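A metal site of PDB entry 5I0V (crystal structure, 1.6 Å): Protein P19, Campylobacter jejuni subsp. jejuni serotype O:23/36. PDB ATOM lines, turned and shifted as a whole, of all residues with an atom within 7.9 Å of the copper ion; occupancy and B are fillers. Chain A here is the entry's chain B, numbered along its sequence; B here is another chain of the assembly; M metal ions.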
ATOM      1  N   LEU A  22      15.272   9.263 -10.788  1.00  0.00           N
ATOM      2  CA  LEU A  22      15.536   9.335 -12.198  1.00  0.00           C
ATOM      3  C   LEU A  22      14.586   8.359 -12.911  1.00  0.00           C
ATOM      4  O   LEU A  22      13.657   7.838 -12.293  1.00  0.00           O
ATOM      5  CB  LEU A  22      17.006   9.027 -12.506  1.00  0.00           C
ATOM      6  CG  LEU A  22      17.580   7.684 -12.008  1.00  0.00           C
ATOM      7  CD1 LEU A  22      18.748   7.223 -12.877  1.00  0.00           C
ATOM      8  CD2 LEU A  22      18.016   7.761 -10.549  1.00  0.00           C
ATOM      9  N   ILE A  25      15.561   2.045 -14.124  1.00  0.00           N
ATOM     10  CA  ILE A  25      16.812   1.452 -14.566  1.00  0.00           C
ATOM     11  C   ILE A  25      16.651  -0.065 -14.702  1.00  0.00           C
ATOM     12  O   ILE A  25      15.651  -0.613 -14.260  1.00  0.00           O
ATOM     13  CB  ILE A  25      17.990   1.854 -13.639  1.00  0.00           C
ATOM     14  CG1 ILE A  25      17.746   1.421 -12.181  1.00  0.00           C
ATOM     15  CG2 ILE A  25      18.185   3.363 -13.710  1.00  0.00           C
ATOM     16  CD1 ILE A  25      18.191   0.007 -11.824  1.00  0.00           C
ATOM     17  N   GLU A  26      17.602  -0.732 -15.349  1.00  0.00           N
ATOM     18  CA  GLU A  26      17.559  -2.187 -15.380  1.00  0.00           C
ATOM     19  C   GLU A  26      18.722  -2.733 -14.557  1.00  0.00           C
ATOM     20  O   GLU A  26      19.872  -2.383 -14.805  1.00  0.00           O
ATOM     21  CB  GLU A  26      17.605  -2.711 -16.809  1.00  0.00           C
ATOM     22  CG  GLU A  26      16.340  -2.453 -17.609  1.00  0.00           C
ATOM     23  CD  GLU A  26      15.233  -3.462 -17.338  1.00  0.00           C
ATOM     24  OE1 GLU A  26      14.718  -4.038 -18.324  1.00  0.00           O
ATOM     25  OE2 GLU A  26      14.852  -3.676 -16.166  1.00  0.00           O
ATOM     26  N   MET A  27      18.390  -3.564 -13.583  1.00  0.00           N
ATOM     27  CA  MET A  27      19.366  -4.092 -12.615  1.00  0.00           C
ATOM     28  C   MET A  27      19.648  -5.579 -12.800  1.00  0.00           C
ATOM     29  O   MET A  27      18.761  -6.358 -13.124  1.00  0.00           O
ATOM     30  CB  MET A  27      18.891  -3.858 -11.177  1.00  0.00           C
ATOM     31  CG  MET A  27      20.033  -3.791 -10.143  1.00  0.00           C
ATOM     32  SD  MET A  27      19.544  -3.895  -8.410  1.00  0.00           S
ATOM     33  CE  MET A  27      19.319  -5.661  -8.253  1.00  0.00           C
ATOM     34  N   ASP A  33      15.001  -6.164  -8.052  1.00  0.00           N
ATOM     35  CA  ASP A  33      14.455  -4.833  -8.268  1.00  0.00           C
ATOM     36  C   ASP A  33      13.249  -4.972  -9.194  1.00  0.00           C
ATOM     37  O   ASP A  33      13.263  -5.808 -10.087  1.00  0.00           O
ATOM     38  CB  ASP A  33      15.511  -3.948  -8.966  1.00  0.00           C
ATOM     39  CG  ASP A  33      15.144  -2.468  -8.979  1.00  0.00           C
ATOM     40  OD1 ASP A  33      14.563  -1.984  -7.990  1.00  0.00           O
ATOM     41  OD2 ASP A  33      15.458  -1.793  -9.992  1.00  0.00           O
ATOM     42  N   HIS A  42      13.336   5.546 -10.694  1.00  0.00           N
ATOM     43  CA  HIS A  42      14.309   4.871  -9.850  1.00  0.00           C
ATOM     44  C   HIS A  42      14.563   5.849  -8.740  1.00  0.00           C
ATOM     45  O   HIS A  42      14.973   6.968  -9.001  1.00  0.00           O
ATOM     46  CB  HIS A  42      15.587   4.536 -10.624  1.00  0.00           C
ATOM     47  CG  HIS A  42      16.506   3.560  -9.880  1.00  0.00           C
ATOM     48  ND1 HIS A  42      16.094   2.332  -9.497  1.00  0.00           N
ATOM     49  CD2 HIS A  42      17.828   3.679  -9.459  1.00  0.00           C
ATOM     50  CE1 HIS A  42      17.097   1.684  -8.884  1.00  0.00           C
ATOM     51  NE2 HIS A  42      18.160   2.502  -8.859  1.00  0.00           N
ATOM     52  N   LEU A  43      14.295   5.441  -7.488  1.00  0.00           N
ATOM     53  CA  LEU A  43      14.538   6.254  -6.322  1.00  0.00           C
ATOM     54  C   LEU A  43      15.888   5.849  -5.735  1.00  0.00           C
ATOM     55  O   LEU A  43      16.143   4.670  -5.576  1.00  0.00           O
ATOM     56  CB  LEU A  43      13.444   6.010  -5.283  1.00  0.00           C
ATOM     57  CG  LEU A  43      13.664   6.616  -3.875  1.00  0.00           C
ATOM     58  CD1 LEU A  43      13.622   8.125  -4.004  1.00  0.00           C
ATOM     59  CD2 LEU A  43      12.559   6.151  -2.931  1.00  0.00           C
ATOM     60  N   GLU A  44      16.707   6.834  -5.420  1.00  0.00           N
ATOM     61  CA  GLU A  44      18.023   6.579  -4.846  1.00  0.00           C
ATOM     62  C   GLU A  44      18.239   7.346  -3.543  1.00  0.00           C
ATOM     63  O   GLU A  44      17.815   8.517  -3.409  1.00  0.00           O
ATOM     64  CB  GLU A  44      19.127   6.984  -5.829  1.00  0.00           C
ATOM     65  CG  GLU A  44      19.126   6.158  -7.098  1.00  0.00           C
ATOM     66  CD  GLU A  44      20.226   6.521  -8.047  1.00  0.00           C
ATOM     67  OE1 GLU A  44      20.851   7.614  -7.918  1.00  0.00           O
ATOM     68  OE2 GLU A  44      20.470   5.718  -8.972  1.00  0.00           O
ATOM     69  N   ALA A  45      18.843   6.657  -2.582  1.00  0.00           N
ATOM     70  CA  ALA A  45      19.339   7.316  -1.384  1.00  0.00           C
ATOM     71  C   ALA A  45      20.840   7.407  -1.587  1.00  0.00           C
ATOM     72  O   ALA A  45      21.502   6.389  -1.830  1.00  0.00           O
ATOM     73  CB  ALA A  45      19.001   6.529  -0.125  1.00  0.00           C
ATOM     74  N   MET A  86      17.843  -1.089  -2.179  1.00  0.00           N
ATOM     75  CA  MET A  86      18.840  -2.139  -2.272  1.00  0.00           C
ATOM     76  C   MET A  86      20.203  -1.565  -2.671  1.00  0.00           C
ATOM     77  O   MET A  86      20.271  -0.620  -3.469  1.00  0.00           O
ATOM     78  CB  MET A  86      18.390  -3.181  -3.306  1.00  0.00           C
ATOM     79  CG  MET A  86      17.095  -3.891  -2.919  1.00  0.00           C
ATOM     80  SD  MET A  86      17.283  -4.930  -1.459  1.00  0.00           S
ATOM     81  CE  MET A  86      15.577  -5.318  -1.060  1.00  0.00           C
ATOM     82  N   PRO A  87      21.304  -2.136  -2.131  1.00  0.00           N
ATOM     83  CA  PRO A  87      22.603  -1.615  -2.516  1.00  0.00           C
ATOM     84  C   PRO A  87      23.005  -2.073  -3.916  1.00  0.00           C
ATOM     85  O   PRO A  87      22.795  -3.245  -4.274  1.00  0.00           O
ATOM     86  CB  PRO A  87      23.555  -2.244  -1.494  1.00  0.00           C
ATOM     87  CG  PRO A  87      22.903  -3.523  -1.101  1.00  0.00           C
ATOM     88  CD  PRO A  87      21.408  -3.297  -1.224  1.00  0.00           C
ATOM     89  N   MET A  88      23.533  -1.140  -4.700  1.00  0.00           N
ATOM     90  CA  MET A  88      23.898  -1.444  -6.082  1.00  0.00           C
ATOM     91  C   MET A  88      24.848  -0.377  -6.585  1.00  0.00           C
ATOM     92  O   MET A  88      25.070   0.619  -5.904  1.00  0.00           O
ATOM     93  CB  MET A  88      22.638  -1.500  -6.964  1.00  0.00           C
ATOM     94  CG  MET A  88      21.942  -0.152  -7.054  1.00  0.00           C
ATOM     95  SD  MET A  88      20.381  -0.247  -7.942  1.00  0.00           S
ATOM     96  CE  MET A  88      19.280  -0.824  -6.662  1.00  0.00           C
ATOM     97  N   VAL A  89      25.391  -0.592  -7.780  1.00  0.00           N
ATOM     98  CA  VAL A  89      26.308   0.371  -8.400  1.00  0.00           C
ATOM     99  C   VAL A  89      25.810   0.782  -9.793  1.00  0.00           C
ATOM    100  O   VAL A  89      25.297  -0.053 -10.568  1.00  0.00           O
ATOM    101  CB  VAL A  89      27.778  -0.141  -8.414  1.00  0.00           C
ATOM    102  CG1 VAL A  89      27.937  -1.373  -9.333  1.00  0.00           C
ATOM    103  CG2 VAL A  89      28.734   0.976  -8.808  1.00  0.00           C
ATOM    104  N   ALA A  90      25.927   2.067 -10.073  1.00  0.00           N
ATOM    105  CA  ALA A  90      25.588   2.632 -11.384  1.00  0.00           C
ATOM    106  C   ALA A  90      26.808   3.384 -11.846  1.00  0.00           C
ATOM    107  O   ALA A  90      27.857   3.344 -11.194  1.00  0.00           O
ATOM    108  CB  ALA A  90      24.387   3.562 -11.256  1.00  0.00           C
ATOM    109  N   ASP A  92      27.432   6.402 -11.719  1.00  0.00           N
ATOM    110  CA  ASP A  92      27.786   7.418 -10.725  1.00  0.00           C
ATOM    111  C   ASP A  92      28.138   6.803  -9.350  1.00  0.00           C
ATOM    112  O   ASP A  92      28.142   7.495  -8.319  1.00  0.00           O
ATOM    113  CB  ASP A  92      26.669   8.495 -10.620  1.00  0.00           C
ATOM    114  CG  ASP A  92      25.373   7.974 -10.011  1.00  0.00           C
ATOM    115  OD1 ASP A  92      25.152   6.749  -9.990  1.00  0.00           O
ATOM    116  OD2 ASP A  92      24.548   8.790  -9.526  1.00  0.00           O
ATOM    117  N   GLY A  93      28.441   5.501  -9.359  1.00  0.00           N
ATOM    118  CA  GLY A  93      28.927   4.792  -8.183  1.00  0.00           C
ATOM    119  C   GLY A  93      27.860   4.109  -7.348  1.00  0.00           C
ATOM    120  O   GLY A  93      26.695   4.059  -7.751  1.00  0.00           O
ATOM    121  N   PRO A  94      28.252   3.574  -6.192  1.00  0.00           N
ATOM    122  CA  PRO A  94      27.347   2.804  -5.347  1.00  0.00           C
ATOM    123  C   PRO A  94      26.276   3.685  -4.699  1.00  0.00           C
ATOM    124  O   PRO A  94      26.515   4.882  -4.415  1.00  0.00           O
ATOM    125  CB  PRO A  94      28.277   2.191  -4.294  1.00  0.00           C
ATOM    126  CG  PRO A  94      29.434   3.143  -4.206  1.00  0.00           C
ATOM    127  CD  PRO A  94      29.621   3.662  -5.611  1.00  0.00           C
ATOM    128  N   HIS A  95      25.088   3.120  -4.513  1.00  0.00           N
ATOM    129  CA  HIS A  95      24.001   3.803  -3.813  1.00  0.00           C
ATOM    130  C   HIS A  95      23.015   2.792  -3.327  1.00  0.00           C
ATOM    131  O   HIS A  95      23.210   1.572  -3.469  1.00  0.00           O
ATOM    132  CB  HIS A  95      23.299   4.788  -4.754  1.00  0.00           C
ATOM    133  CG  HIS A  95      22.734   4.110  -5.984  1.00  0.00           C
ATOM    134  ND1 HIS A  95      23.479   3.906  -7.093  1.00  0.00           N
ATOM    135  CD2 HIS A  95      21.474   3.575  -6.236  1.00  0.00           C
ATOM    136  CE1 HIS A  95      22.720   3.271  -8.022  1.00  0.00           C
ATOM    137  NE2 HIS A  95      21.503   3.061  -7.486  1.00  0.00           N
ATOM    138  N   TYR A  96      21.922   3.271  -2.758  1.00  0.00           N
ATOM    139  CA  TYR A  96      20.799   2.405  -2.425  1.00  0.00           C
ATOM    140  C   TYR A  96      19.625   2.839  -3.275  1.00  0.00           C
ATOM    141  O   TYR A  96      19.307   4.017  -3.323  1.00  0.00           O
ATOM    142  CB  TYR A  96      20.439   2.502  -0.946  1.00  0.00           C
ATOM    143  CG  TYR A  96      21.570   2.123  -0.007  1.00  0.00           C
ATOM    144  CD1 TYR A  96      21.711   0.820   0.456  1.00  0.00           C
ATOM    145  CD2 TYR A  96      22.485   3.092   0.439  1.00  0.00           C
ATOM    146  CE1 TYR A  96      22.723   0.463   1.331  1.00  0.00           C
ATOM    147  CE2 TYR A  96      23.509   2.730   1.332  1.00  0.00           C
ATOM    148  CZ  TYR A  96      23.617   1.433   1.769  1.00  0.00           C
ATOM    149  OH  TYR A  96      24.648   1.099   2.634  1.00  0.00           O
ATOM    150  N   GLY A  97      19.005   1.887  -3.956  1.00  0.00           N
ATOM    151  CA  GLY A  97      18.000   2.231  -4.970  1.00  0.00           C
ATOM    152  C   GLY A  97      16.857   1.258  -5.058  1.00  0.00           C
ATOM    153  O   GLY A  97      16.935   0.150  -4.533  1.00  0.00           O
ATOM    154  N   ALA A  98      15.790   1.708  -5.715  1.00  0.00           N
ATOM    155  CA  ALA A  98      14.653   0.846  -6.067  1.00  0.00           C
ATOM    156  C   ALA A  98      13.888   1.457  -7.212  1.00  0.00           C
ATOM    157  O   ALA A  98      13.615   2.647  -7.191  1.00  0.00           O
ATOM    158  CB  ALA A  98      13.696   0.668  -4.883  1.00  0.00           C
ATOM    159  N   ASN A  99      13.540   0.649  -8.209  1.00  0.00           N
ATOM    160  CA  ASN A  99      12.524   1.061  -9.180  1.00  0.00           C
ATOM    161  C   ASN A  99      11.157   1.081  -8.503  1.00  0.00           C
ATOM    162  O   ASN A  99      10.829   0.226  -7.676  1.00  0.00           O
ATOM    163  CB  ASN A  99      12.491   0.095 -10.375  1.00  0.00           C
ATOM    164  CG  ASN A  99      13.523   0.409 -11.459  1.00  0.00           C
ATOM    165  OD1 ASN A  99      14.270   1.396 -11.451  1.00  0.00           O
ATOM    166  ND2 ASN A  99      13.568  -0.487 -12.445  1.00  0.00           N
ATOM    167  N   GLY B 130      23.668  -5.159  -6.373  1.00  0.00           N
ATOM    168  CA  GLY B 130      23.235  -4.976  -7.751  1.00  0.00           C
ATOM    169  C   GLY B 130      24.102  -4.104  -8.653  1.00  0.00           C
ATOM    170  O   GLY B 130      25.039  -3.442  -8.197  1.00  0.00           O
ATOM    171  N   ARG B 131      23.807  -4.152  -9.943  1.00  0.00           N
ATOM    172  CA  ARG B 131      24.414  -3.207 -10.900  1.00  0.00           C
ATOM    173  C   ARG B 131      23.459  -2.804 -11.990  1.00  0.00           C
ATOM    174  O   ARG B 131      22.691  -3.633 -12.509  1.00  0.00           O
ATOM    175  CB  ARG B 131      25.730  -3.707 -11.500  1.00  0.00           C
ATOM    176  CG  ARG B 131      25.671  -5.007 -12.261  1.00  0.00           C
ATOM    177  CD  ARG B 131      26.929  -5.229 -13.110  1.00  0.00           C
ATOM    178  NE  ARG B 131      26.658  -6.325 -14.014  1.00  0.00           N
ATOM    179  CZ  ARG B 131      26.670  -6.246 -15.334  1.00  0.00           C
ATOM    180  NH1 ARG B 131      27.002  -5.125 -15.960  1.00  0.00           N
ATOM    181  NH2 ARG B 131      26.379  -7.330 -16.027  1.00  0.00           N
ATOM    182  N   HIS B 132      23.468  -1.514 -12.323  1.00  0.00           N
ATOM    183  CA  HIS B 132      22.681  -1.016 -13.432  1.00  0.00           C
ATOM    184  C   HIS B 132      23.306  -1.532 -14.695  1.00  0.00           C
ATOM    185  O   HIS B 132      24.527  -1.548 -14.829  1.00  0.00           O
ATOM    186  CB  HIS B 132      22.685   0.506 -13.469  1.00  0.00           C
ATOM    187  CG  HIS B 132      21.953   1.174 -12.315  1.00  0.00           C
ATOM    188  ND1 HIS B 132      21.444   2.418 -12.436  1.00  0.00           N
ATOM    189  CD2 HIS B 132      21.670   0.767 -11.014  1.00  0.00           C
ATOM    190  CE1 HIS B 132      20.884   2.794 -11.273  1.00  0.00           C
ATOM    191  NE2 HIS B 132      20.988   1.771 -10.407  1.00  0.00           N
ATOM    192  N   ASP B 134      21.305  -0.844 -17.820  1.00  0.00           N
ATOM    193  CA  ASP B 134      20.706  -0.023 -18.885  1.00  0.00           C
ATOM    194  C   ASP B 134      21.776   0.856 -19.543  1.00  0.00           C
ATOM    195  O   ASP B 134      22.830   1.091 -18.959  1.00  0.00           O
ATOM    196  CB  ASP B 134      19.601   0.873 -18.343  1.00  0.00           C
ATOM    197  CG  ASP B 134      20.034   1.609 -17.092  1.00  0.00           C
ATOM    198  OD1 ASP B 134      20.099   0.928 -16.031  1.00  0.00           O
ATOM    199  OD2 ASP B 134      20.334   2.828 -17.192  1.00  0.00           O
ATOM    200  N   THR B 137      22.744   4.496 -17.642  1.00  0.00           N
ATOM    201  CA  THR B 137      23.385   4.534 -16.315  1.00  0.00           C
ATOM    202  C   THR B 137      24.177   3.283 -15.972  1.00  0.00           C
ATOM    203  O   THR B 137      24.728   3.188 -14.852  1.00  0.00           O
ATOM    204  CB  THR B 137      22.361   4.770 -15.179  1.00  0.00           C
ATOM    205  OG1 THR B 137      21.555   3.595 -14.999  1.00  0.00           O
ATOM    206  CG2 THR B 137      21.467   5.970 -15.458  1.00  0.00           C
HETATM  207 CU    CU M   1      20.080   1.946  -8.508  1.00  0.00          CU
HETATM  208 FE    FE M   2      22.542   8.474  -8.630  1.00  0.00          FE
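The side-chain hydroxyl of Thr 137 of chain B is in hydrogen-bond range of a ring nitrogen (ND1) of His 132 of chain B (2.8 Å). NE2 of His 95 sits close to OE2 of Glu 44 (3.2 Å). The backbone NH (N) of His 132 of chain B lies within hydrogen-bond range of the backbone carbonyl oxygen (O) of Val 89, at 2.9 Å. A ring nitrogen (ND1) of His 95 lies within hydrogen-bond range of the backbone carbonyl oxygen of Gly 93 (3.3 Å). OD1 of Asn 99 is in hydrogen-bond range of ND1 of His 42 (2.8 Å). The backbone carbonyl oxygen (O) of Leu 22 lies within hydrogen-bond range of the backbone NH (N) of His 42, 2.8 Å away. A ring nitrogen (ND1) of His 42 sits close to the backbone carbonyl oxygen of Ala 98, at 3.4 Å.
Merely in contact with the copper ion: Glu 44 (3.8 Å).
The copper ion is bound by a ring nitrogen (NE2) of His 42 (2.0 Å), a ring nitrogen (NE2) of His 95 (2.1 Å), a ring nitrogen (NE2) of His 132 of chain B (2.1 Å) and the side-chain sulfur (SD) of Met 88 (2.3 Å). The copper ion has four donor atoms within binding distance.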
